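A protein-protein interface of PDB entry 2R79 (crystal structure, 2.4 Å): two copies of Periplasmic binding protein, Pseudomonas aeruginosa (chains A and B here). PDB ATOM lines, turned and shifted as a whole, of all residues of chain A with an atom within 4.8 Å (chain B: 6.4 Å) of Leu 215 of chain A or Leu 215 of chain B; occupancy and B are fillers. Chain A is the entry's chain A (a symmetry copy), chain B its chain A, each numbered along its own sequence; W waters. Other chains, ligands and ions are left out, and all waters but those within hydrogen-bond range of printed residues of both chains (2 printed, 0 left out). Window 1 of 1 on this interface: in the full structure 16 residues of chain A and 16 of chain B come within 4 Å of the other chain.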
ATOM      1  N   ARG A 211      23.456 -30.196   5.820  1.00  0.00           N
ATOM      2  CA  ARG A 211      23.097 -31.060   6.944  1.00  0.00           C
ATOM      3  C   ARG A 211      23.216 -30.331   8.268  1.00  0.00           C
ATOM      4  O   ARG A 211      22.312 -30.398   9.112  1.00  0.00           O
ATOM      5  CB  ARG A 211      23.996 -32.289   7.008  1.00  0.00           C
ATOM      6  CG  ARG A 211      23.880 -33.196   5.825  1.00  0.00           C
ATOM      7  CD  ARG A 211      24.512 -34.547   6.075  1.00  0.00           C
ATOM      8  NE  ARG A 211      24.297 -35.369   4.895  1.00  0.00           N
ATOM      9  CZ  ARG A 211      24.954 -35.224   3.748  1.00  0.00           C
ATOM     10  NH1 ARG A 211      25.895 -34.301   3.621  1.00  0.00           N
ATOM     11  NH2 ARG A 211      24.623 -35.964   2.702  1.00  0.00           N
ATOM     12  N   ALA A 212      24.344 -29.648   8.446  1.00  0.00           N
ATOM     13  CA  ALA A 212      24.604 -28.922   9.675  1.00  0.00           C
ATOM     14  C   ALA A 212      23.554 -27.846   9.906  1.00  0.00           C
ATOM     15  O   ALA A 212      23.037 -27.713  11.011  1.00  0.00           O
ATOM     16  CB  ALA A 212      25.997 -28.303   9.637  1.00  0.00           C
ATOM     17  N   ALA A 213      23.237 -27.080   8.866  1.00  0.00           N
ATOM     18  CA  ALA A 213      22.238 -26.030   8.997  1.00  0.00           C
ATOM     19  C   ALA A 213      20.885 -26.632   9.356  1.00  0.00           C
ATOM     20  O   ALA A 213      20.160 -26.109  10.201  1.00  0.00           O
ATOM     21  CB  ALA A 213      22.130 -25.252   7.712  1.00  0.00           C
ATOM     22  N   LEU A 214      20.553 -27.743   8.718  1.00  0.00           N
ATOM     23  CA  LEU A 214      19.285 -28.404   8.975  1.00  0.00           C
ATOM     24  C   LEU A 214      19.150 -28.775  10.449  1.00  0.00           C
ATOM     25  O   LEU A 214      18.109 -28.549  11.065  1.00  0.00           O
ATOM     26  CB  LEU A 214      19.176 -29.668   8.123  1.00  0.00           C
ATOM     27  CG  LEU A 214      17.860 -30.440   8.223  1.00  0.00           C
ATOM     28  CD1 LEU A 214      16.773 -29.675   7.491  1.00  0.00           C
ATOM     29  CD2 LEU A 214      18.030 -31.825   7.623  1.00  0.00           C
ATOM     30  N   LEU A 215      20.211 -29.346  11.008  1.00  0.00           N
ATOM     31  CA  LEU A 215      20.196 -29.770  12.400  1.00  0.00           C
ATOM     32  C   LEU A 215      20.205 -28.594  13.365  1.00  0.00           C
ATOM     33  O   LEU A 215      19.581 -28.654  14.430  1.00  0.00           O
ATOM     34  CB  LEU A 215      21.377 -30.699  12.659  1.00  0.00           C
ATOM     35  CG  LEU A 215      21.220 -32.033  11.912  1.00  0.00           C
ATOM     36  CD1 LEU A 215      22.551 -32.747  11.780  1.00  0.00           C
ATOM     37  CD2 LEU A 215      20.215 -32.893  12.656  1.00  0.00           C
ATOM     38  N   LYS A 216      20.902 -27.522  12.993  1.00  0.00           N
ATOM     39  CA  LYS A 216      20.953 -26.340  13.835  1.00  0.00           C
ATOM     40  C   LYS A 216      19.566 -25.773  14.038  1.00  0.00           C
ATOM     41  O   LYS A 216      19.145 -25.516  15.166  1.00  0.00           O
ATOM     42  CB  LYS A 216      21.816 -25.258  13.208  1.00  0.00           C
ATOM     43  CG  LYS A 216      23.271 -25.382  13.501  1.00  0.00           C
ATOM     44  CD  LYS A 216      23.988 -24.137  13.050  1.00  0.00           C
ATOM     45  CE  LYS A 216      25.449 -24.180  13.437  1.00  0.00           C
ATOM     46  NZ  LYS A 216      26.054 -22.843  13.230  1.00  0.00           N
ATOM     47  N   GLN A 217      18.852 -25.588  12.935  1.00  0.00           N
ATOM     48  CA  GLN A 217      17.519 -25.014  12.981  1.00  0.00           C
ATOM     49  C   GLN A 217      16.386 -25.981  13.288  1.00  0.00           C
ATOM     50  O   GLN A 217      15.271 -25.551  13.552  1.00  0.00           O
ATOM     51  CB  GLN A 217      17.246 -24.278  11.669  1.00  0.00           C
ATOM     52  CG  GLN A 217      18.310 -23.231  11.381  1.00  0.00           C
ATOM     53  CD  GLN A 217      17.935 -22.292  10.259  1.00  0.00           C
ATOM     54  OE1 GLN A 217      16.872 -21.674  10.285  1.00  0.00           O
ATOM     55  NE2 GLN A 217      18.815 -22.168   9.270  1.00  0.00           N
ATOM     56  N   ASN A 218      16.668 -27.280  13.270  1.00  0.00           N
ATOM     57  CA  ASN A 218      15.640 -28.288  13.545  1.00  0.00           C
ATOM     58  C   ASN A 218      16.249 -29.434  14.354  1.00  0.00           C
ATOM     59  O   ASN A 218      16.266 -30.580  13.906  1.00  0.00           O
ATOM     60  CB  ASN A 218      15.091 -28.819  12.221  1.00  0.00           C
ATOM     61  CG  ASN A 218      14.731 -27.704  11.252  1.00  0.00           C
ATOM     62  OD1 ASN A 218      13.722 -27.024  11.420  1.00  0.00           O
ATOM     63  ND2 ASN A 218      15.567 -27.505  10.238  1.00  0.00           N
ATOM     64  N   PRO A 219      16.741 -29.135  15.569  1.00  0.00           N
ATOM     65  CA  PRO A 219      17.372 -30.104  16.478  1.00  0.00           C
ATOM     66  C   PRO A 219      16.576 -31.388  16.657  1.00  0.00           C
ATOM     67  O   PRO A 219      17.145 -32.459  16.866  1.00  0.00           O
ATOM     68  CB  PRO A 219      17.500 -29.325  17.785  1.00  0.00           C
ATOM     69  CG  PRO A 219      17.593 -27.904  17.330  1.00  0.00           C
ATOM     70  CD  PRO A 219      16.556 -27.840  16.246  1.00  0.00           C
ATOM     71  N   LEU A 221      15.254 -33.241  14.586  1.00  0.00           N
ATOM     72  CA  LEU A 221      15.501 -34.262  13.569  1.00  0.00           C
ATOM     73  C   LEU A 221      16.651 -35.194  13.929  1.00  0.00           C
ATOM     74  O   LEU A 221      16.767 -36.290  13.374  1.00  0.00           O
ATOM     75  CB  LEU A 221      15.782 -33.613  12.213  1.00  0.00           C
ATOM     76  CG  LEU A 221      14.718 -32.626  11.723  1.00  0.00           C
ATOM     77  CD1 LEU A 221      15.077 -32.138  10.329  1.00  0.00           C
ATOM     78  CD2 LEU A 221      13.354 -33.290  11.726  1.00  0.00           C
ATOM     79  N   ALA A 222      17.496 -34.764  14.863  1.00  0.00           N
ATOM     80  CA  ALA A 222      18.637 -35.571  15.289  1.00  0.00           C
ATOM     81  C   ALA A 222      18.250 -36.931  15.874  1.00  0.00           C
ATOM     82  O   ALA A 222      19.040 -37.872  15.836  1.00  0.00           O
ATOM     83  CB  ALA A 222      19.473 -34.796  16.291  1.00  0.00           C
ATOM     84  N   LEU A 232      20.662 -38.409   5.842  1.00  0.00           N
ATOM     85  CA  LEU A 232      20.129 -37.095   5.545  1.00  0.00           C
ATOM     86  C   LEU A 232      20.744 -36.870   4.166  1.00  0.00           C
ATOM     87  O   LEU A 232      21.905 -36.477   4.054  1.00  0.00           O
ATOM     88  CB  LEU A 232      20.650 -36.051   6.531  1.00  0.00           C
ATOM     89  CG  LEU A 232      20.235 -36.205   7.994  1.00  0.00           C
ATOM     90  CD1 LEU A 232      20.780 -35.030   8.793  1.00  0.00           C
ATOM     91  CD2 LEU A 232      18.713 -36.269   8.098  1.00  0.00           C
ATOM     92  N   GLY B 152      32.275 -36.635  16.288  1.00  0.00           N
ATOM     93  CA  GLY B 152      31.192 -35.944  16.970  1.00  0.00           C
ATOM     94  C   GLY B 152      30.679 -36.574  18.248  1.00  0.00           C
ATOM     95  O   GLY B 152      29.813 -36.010  18.908  1.00  0.00           O
ATOM     96  N   ALA B 210      32.261 -32.182  10.687  1.00  0.00           N
ATOM     97  CA  ALA B 210      32.469 -32.183  12.120  1.00  0.00           C
ATOM     98  C   ALA B 210      31.292 -31.493  12.802  1.00  0.00           C
ATOM     99  O   ALA B 210      30.808 -31.965  13.825  1.00  0.00           O
ATOM    100  CB  ALA B 210      33.779 -31.472  12.467  1.00  0.00           C
ATOM    101  N   ARG B 211      30.826 -30.383  12.231  1.00  0.00           N
ATOM    102  CA  ARG B 211      29.703 -29.647  12.808  1.00  0.00           C
ATOM    103  C   ARG B 211      28.433 -30.475  12.805  1.00  0.00           C
ATOM    104  O   ARG B 211      27.720 -30.546  13.815  1.00  0.00           O
ATOM    105  CB  ARG B 211      29.423 -28.365  12.033  1.00  0.00           C
ATOM    106  CG  ARG B 211      30.540 -27.371  12.067  1.00  0.00           C
ATOM    107  CD  ARG B 211      30.105 -26.003  11.591  1.00  0.00           C
ATOM    108  NE  ARG B 211      31.239 -25.102  11.717  1.00  0.00           N
ATOM    109  CZ  ARG B 211      32.292 -25.100  10.903  1.00  0.00           C
ATOM    110  NH1 ARG B 211      32.355 -25.937   9.879  1.00  0.00           N
ATOM    111  NH2 ARG B 211      33.316 -24.300  11.154  1.00  0.00           N
ATOM    112  N   ALA B 212      28.151 -31.085  11.656  1.00  0.00           N
ATOM    113  CA  ALA B 212      26.954 -31.892  11.501  1.00  0.00           C
ATOM    114  C   ALA B 212      26.952 -33.058  12.477  1.00  0.00           C
ATOM    115  O   ALA B 212      25.943 -33.323  13.123  1.00  0.00           O
ATOM    116  CB  ALA B 212      26.844 -32.400  10.067  1.00  0.00           C
ATOM    117  N   ALA B 213      28.080 -33.754  12.587  1.00  0.00           N
ATOM    118  CA  ALA B 213      28.168 -34.883  13.501  1.00  0.00           C
ATOM    119  C   ALA B 213      27.957 -34.415  14.936  1.00  0.00           C
ATOM    120  O   ALA B 213      27.263 -35.060  15.720  1.00  0.00           O
ATOM    121  CB  ALA B 213      29.509 -35.554  13.371  1.00  0.00           C
ATOM    122  N   LEU B 214      28.551 -33.281  15.274  1.00  0.00           N
ATOM    123  CA  LEU B 214      28.424 -32.740  16.616  1.00  0.00           C
ATOM    124  C   LEU B 214      26.961 -32.507  16.977  1.00  0.00           C
ATOM    125  O   LEU B 214      26.514 -32.861  18.068  1.00  0.00           O
ATOM    126  CB  LEU B 214      29.187 -31.421  16.718  1.00  0.00           C
ATOM    127  CG  LEU B 214      29.214 -30.759  18.096  1.00  0.00           C
ATOM    128  CD1 LEU B 214      30.145 -31.537  19.007  1.00  0.00           C
ATOM    129  CD2 LEU B 214      29.682 -29.320  17.967  1.00  0.00           C
ATOM    130  N   LEU B 215      26.218 -31.909  16.052  1.00  0.00           N
ATOM    131  CA  LEU B 215      24.815 -31.607  16.287  1.00  0.00           C
ATOM    132  C   LEU B 215      23.948 -32.857  16.307  1.00  0.00           C
ATOM    133  O   LEU B 215      22.978 -32.934  17.070  1.00  0.00           O
ATOM    134  CB  LEU B 215      24.325 -30.618  15.235  1.00  0.00           C
ATOM    135  CG  LEU B 215      24.986 -29.241  15.404  1.00  0.00           C
ATOM    136  CD1 LEU B 215      24.878 -28.421  14.133  1.00  0.00           C
ATOM    137  CD2 LEU B 215      24.327 -28.524  16.568  1.00  0.00           C
ATOM    138  N   LYS B 216      24.297 -33.839  15.479  1.00  0.00           N
ATOM    139  CA  LYS B 216      23.546 -35.081  15.439  1.00  0.00           C
ATOM    140  C   LYS B 216      23.581 -35.765  16.788  1.00  0.00           C
ATOM    141  O   LYS B 216      22.545 -36.147  17.331  1.00  0.00           O
ATOM    142  CB  LYS B 216      24.126 -36.039  14.412  1.00  0.00           C
ATOM    143  CG  LYS B 216      23.624 -35.833  13.025  1.00  0.00           C
ATOM    144  CD  LYS B 216      24.062 -36.978  12.151  1.00  0.00           C
ATOM    145  CE  LYS B 216      23.473 -36.860  10.763  1.00  0.00           C
ATOM    146  NZ  LYS B 216      23.692 -38.126  10.024  1.00  0.00           N
ATOM    147  N   GLN B 217      24.783 -35.908  17.330  1.00  0.00           N
ATOM    148  CA  GLN B 217      24.966 -36.581  18.604  1.00  0.00           C
ATOM    149  C   GLN B 217      24.749 -35.730  19.846  1.00  0.00           C
ATOM    150  O   GLN B 217      24.675 -36.262  20.945  1.00  0.00           O
ATOM    151  CB  GLN B 217      26.354 -37.221  18.637  1.00  0.00           C
ATOM    152  CG  GLN B 217      26.567 -38.158  17.459  1.00  0.00           C
ATOM    153  CD  GLN B 217      27.797 -39.023  17.600  1.00  0.00           C
ATOM    154  OE1 GLN B 217      27.966 -39.718  18.601  1.00  0.00           O
ATOM    155  NE2 GLN B 217      28.661 -38.997  16.589  1.00  0.00           N
ATOM    156  N   ASN B 218      24.631 -34.417  19.676  1.00  0.00           N
ATOM    157  CA  ASN B 218      24.428 -33.514  20.813  1.00  0.00           C
ATOM    158  C   ASN B 218      23.460 -32.400  20.416  1.00  0.00           C
ATOM    159  O   ASN B 218      23.814 -31.221  20.438  1.00  0.00           O
ATOM    160  CB  ASN B 218      25.772 -32.915  21.224  1.00  0.00           C
ATOM    161  CG  ASN B 218      26.862 -33.967  21.356  1.00  0.00           C
ATOM    162  OD1 ASN B 218      26.887 -34.732  22.317  1.00  0.00           O
ATOM    163  ND2 ASN B 218      27.762 -34.017  20.379  1.00  0.00           N
ATOM    164  N   PRO B 219      22.213 -32.764  20.066  1.00  0.00           N
ATOM    165  CA  PRO B 219      21.156 -31.831  19.647  1.00  0.00           C
ATOM    166  C   PRO B 219      20.995 -30.630  20.566  1.00  0.00           C
ATOM    167  O   PRO B 219      20.630 -29.540  20.123  1.00  0.00           O
ATOM    168  CB  PRO B 219      19.905 -32.707  19.628  1.00  0.00           C
ATOM    169  CG  PRO B 219      20.447 -34.073  19.354  1.00  0.00           C
ATOM    170  CD  PRO B 219      21.666 -34.122  20.229  1.00  0.00           C
ATOM    171  N   GLY B 220      21.267 -30.831  21.849  1.00  0.00           N
ATOM    172  CA  GLY B 220      21.141 -29.751  22.805  1.00  0.00           C
ATOM    173  C   GLY B 220      22.023 -28.547  22.533  1.00  0.00           C
ATOM    174  O   GLY B 220      21.741 -27.467  23.032  1.00  0.00           O
ATOM    175  N   LEU B 221      23.087 -28.710  21.754  1.00  0.00           N
ATOM    176  CA  LEU B 221      23.981 -27.591  21.461  1.00  0.00           C
ATOM    177  C   LEU B 221      23.396 -26.610  20.452  1.00  0.00           C
ATOM    178  O   LEU B 221      23.847 -25.466  20.357  1.00  0.00           O
ATOM    179  CB  LEU B 221      25.329 -28.100  20.948  1.00  0.00           C
ATOM    180  CG  LEU B 221      26.034 -29.118  21.850  1.00  0.00           C
ATOM    181  CD1 LEU B 221      27.397 -29.457  21.269  1.00  0.00           C
ATOM    182  CD2 LEU B 221      26.172 -28.559  23.254  1.00  0.00           C
ATOM    183  N   ALA B 222      22.389 -27.054  19.706  1.00  0.00           N
ATOM    184  CA  ALA B 222      21.749 -26.205  18.704  1.00  0.00           C
ATOM    185  C   ALA B 222      21.125 -24.931  19.280  1.00  0.00           C
ATOM    186  O   ALA B 222      20.983 -23.935  18.575  1.00  0.00           O
ATOM    187  CB  ALA B 222      20.701 -26.998  17.946  1.00  0.00           C
ATOM    188  N   ALA B 227      25.865 -21.980  18.358  1.00  0.00           N
ATOM    189  CA  ALA B 227      25.217 -22.559  17.181  1.00  0.00           C
ATOM    190  C   ALA B 227      24.400 -21.505  16.434  1.00  0.00           C
ATOM    191  O   ALA B 227      24.426 -21.440  15.205  1.00  0.00           O
ATOM    192  CB  ALA B 227      24.311 -23.731  17.590  1.00  0.00           C
ATOM    193  N   LEU B 232      30.585 -22.431  15.691  1.00  0.00           N
ATOM    194  CA  LEU B 232      31.051 -23.751  16.065  1.00  0.00           C
ATOM    195  C   LEU B 232      32.343 -23.812  15.256  1.00  0.00           C
ATOM    196  O   LEU B 232      32.321 -24.107  14.061  1.00  0.00           O
ATOM    197  CB  LEU B 232      30.081 -24.833  15.593  1.00  0.00           C
ATOM    198  CG  LEU B 232      28.684 -24.836  16.211  1.00  0.00           C
ATOM    199  CD1 LEU B 232      27.905 -26.031  15.679  1.00  0.00           C
ATOM    200  CD2 LEU B 232      28.787 -24.894  17.733  1.00  0.00           C
ATOM    201  N   THR B 280      26.653 -21.585   8.964  1.00  0.00           N
ATOM    202  CA  THR B 280      25.235 -21.856   9.185  1.00  0.00           C
ATOM    203  C   THR B 280      24.694 -21.124  10.411  1.00  0.00           C
ATOM    204  O   THR B 280      25.449 -20.769  11.313  1.00  0.00           O
ATOM    205  CB  THR B 280      24.989 -23.369   9.341  1.00  0.00           C
ATOM    206  OG1 THR B 280      25.797 -23.882  10.411  1.00  0.00           O
ATOM    207  CG2 THR B 280      25.342 -24.095   8.048  1.00  0.00           C
ATOM    208  N   THR B 282      20.829 -20.345  13.041  1.00  0.00           N
ATOM    209  CA  THR B 282      19.615 -20.912  13.625  1.00  0.00           C
ATOM    210  C   THR B 282      18.554 -19.835  13.853  1.00  0.00           C
ATOM    211  O   THR B 282      17.386 -20.013  13.494  1.00  0.00           O
ATOM    212  CB  THR B 282      19.902 -21.593  14.979  1.00  0.00           C
ATOM    213  OG1 THR B 282      20.834 -22.664  14.792  1.00  0.00           O
ATOM    214  CG2 THR B 282      18.615 -22.149  15.574  1.00  0.00           C
HETATM  215  O   HOH W   1      27.607 -22.279  15.291  1.00  0.00           O
HETATM  216  O   HOH W   2      21.483 -38.747   8.717  1.00  0.00           O
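Of chain B, only Ala 212 (3.7 Å), Leu 215 (3.9 Å) and Lys 216 (3.5 Å) come within 4 Å of Leu 215 of chain A. Leu 215 of chain B touches just these residues of chain A: Ala 212, Leu 215 and Lys 216. Of the printed residues of chain A, Thr 280 of chain B touches Ala 213 (3.4 Å) and Lys 216 (2.9 Å). Of the printed residues of chain B, Ala 222 of chain A touches Lys 216 (3.5 Å) and Pro 219 (3.3 Å). Leu 221 of chain B touches none of the printed residues of chain A. Arg 211 of chain A touches none of the printed residues of chain B. The nearest residue of chain A that does not touch Leu 215 of chain B is Ala 222 of chain A (4.04 Å).
Among the printed residues, merely in contact across the chains: Ala 222 of chain A with Pro 219 of chain B (3.3 Å), Pro 219 of chain A with Ala 222 of chain B (3.3 Å), Ala 213 of chain A with Thr 280 of chain B (3.4 Å), Gln 217 of chain A with Thr 282 of chain B (3.5 Å), Lys 216 of chain A with Leu 215 of chain B (3.5 Å), Leu 215 of chain A with Lys 216 of chain B (3.5 Å), Ala 222 of chain A with Lys 216 of chain B (3.5 Å), Lys 216 of chain A with Ala 222 of chain B (3.5 Å), Ala 212 of chain A with Leu 215 of chain B (3.7 Å), Leu 215 of chain A with Ala 212 of chain B (3.7 Å), Leu 232 of chain A with Lys 216 of chain B (3.8 Å), Lys 216 of chain A with Leu 232 of chain B (3.8 Å), Pro 219 of chain A with Pro 219 of chain B (3.9 Å) and Leu 215 of chain A with Leu 215 of chain B (3.9 Å).
Printed residues of chain B that touch a printed residue of chain A: Ala 212, Leu 215, Lys 216, Pro 219, Ala 222, Ala 227, Leu 232, Thr 280 and Thr 282. Hydrophobic or aromatic side chains of chain B that line the printed part of chain A: Leu 215, Pro 219, Ala 222 and Leu 232. Of the 12 printed residues of chain A, 8 touch a printed residue of chain B. Printed residues of chain A that touch a printed residue of chain B: Ala 212, Ala 213, Leu 215, Lys 216, Gln 217, Pro 219, Ala 222 and Leu 232. Hydrophobic or aromatic side chains of chain A within 4 Å of the printed part of chain B: Ala 213, Leu 215, Pro 219, Ala 222 and Leu 232. Among the printed residues, 17 pairs touch across the chains. Among the printed residues, no Asp or Glu carboxylate lies within 4 Å of a Lys or Arg side-chain nitrogen of the other chain.
Water W2 bridges NZ of Lys 216 of chain B and N of Leu 232 of chain A. Water W1 lies within hydrogen-bond range of the side-chain amino group of Lys 216 of chain A (2.6 Å), the backbone NH of Leu 232 of chain B (3.0 Å) and the backbone carbonyl oxygen of Ala 227 of chain B (3.3 Å).
Ala 212 of chain A touches Leu 215 of chain B, and with the chains exchanged Leu 215 of chain A touches Ala 212 of chain B. Leu 215 of chain B touches its own counterpart, Leu 215 of chain A. Leu 215 of chain A touches Lys 216 of chain B, and with the chains exchanged Lys 216 of chain A touches Leu 215 of chain B. Pro 219 of chain A touches Ala 222 of chain B, and with the chains exchanged Ala 222 of chain A touches Pro 219 of chain B. Of the 17 pairs that touch across the chains among the printed residues, 12 have their exchanged pair printed and touching as well.
The guanidinium group (NE) of Arg 211 of chain A is in hydrogen-bond range of the backbone carbonyl oxygen (O) of Leu 232 of chain A (2.8 Å). NE of Arg 211 of chain B lies within hydrogen-bond range of O of Leu 232 of chain B (2.8 Å).
The backbone carbonyl oxygen of Lys 216 of chain A lies close to the side-chain hydroxyl of Thr 282 of chain B. The backbone carbonyl oxygen (O) of Ala 227 of chain B sits at hydrogen-bond distance from the side-chain amino group (NZ) of Lys 216 of chain A (2.9 Å). O of Thr 280 of chain B lies within hydrogen-bond range of NZ of Lys 216 of chain A.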
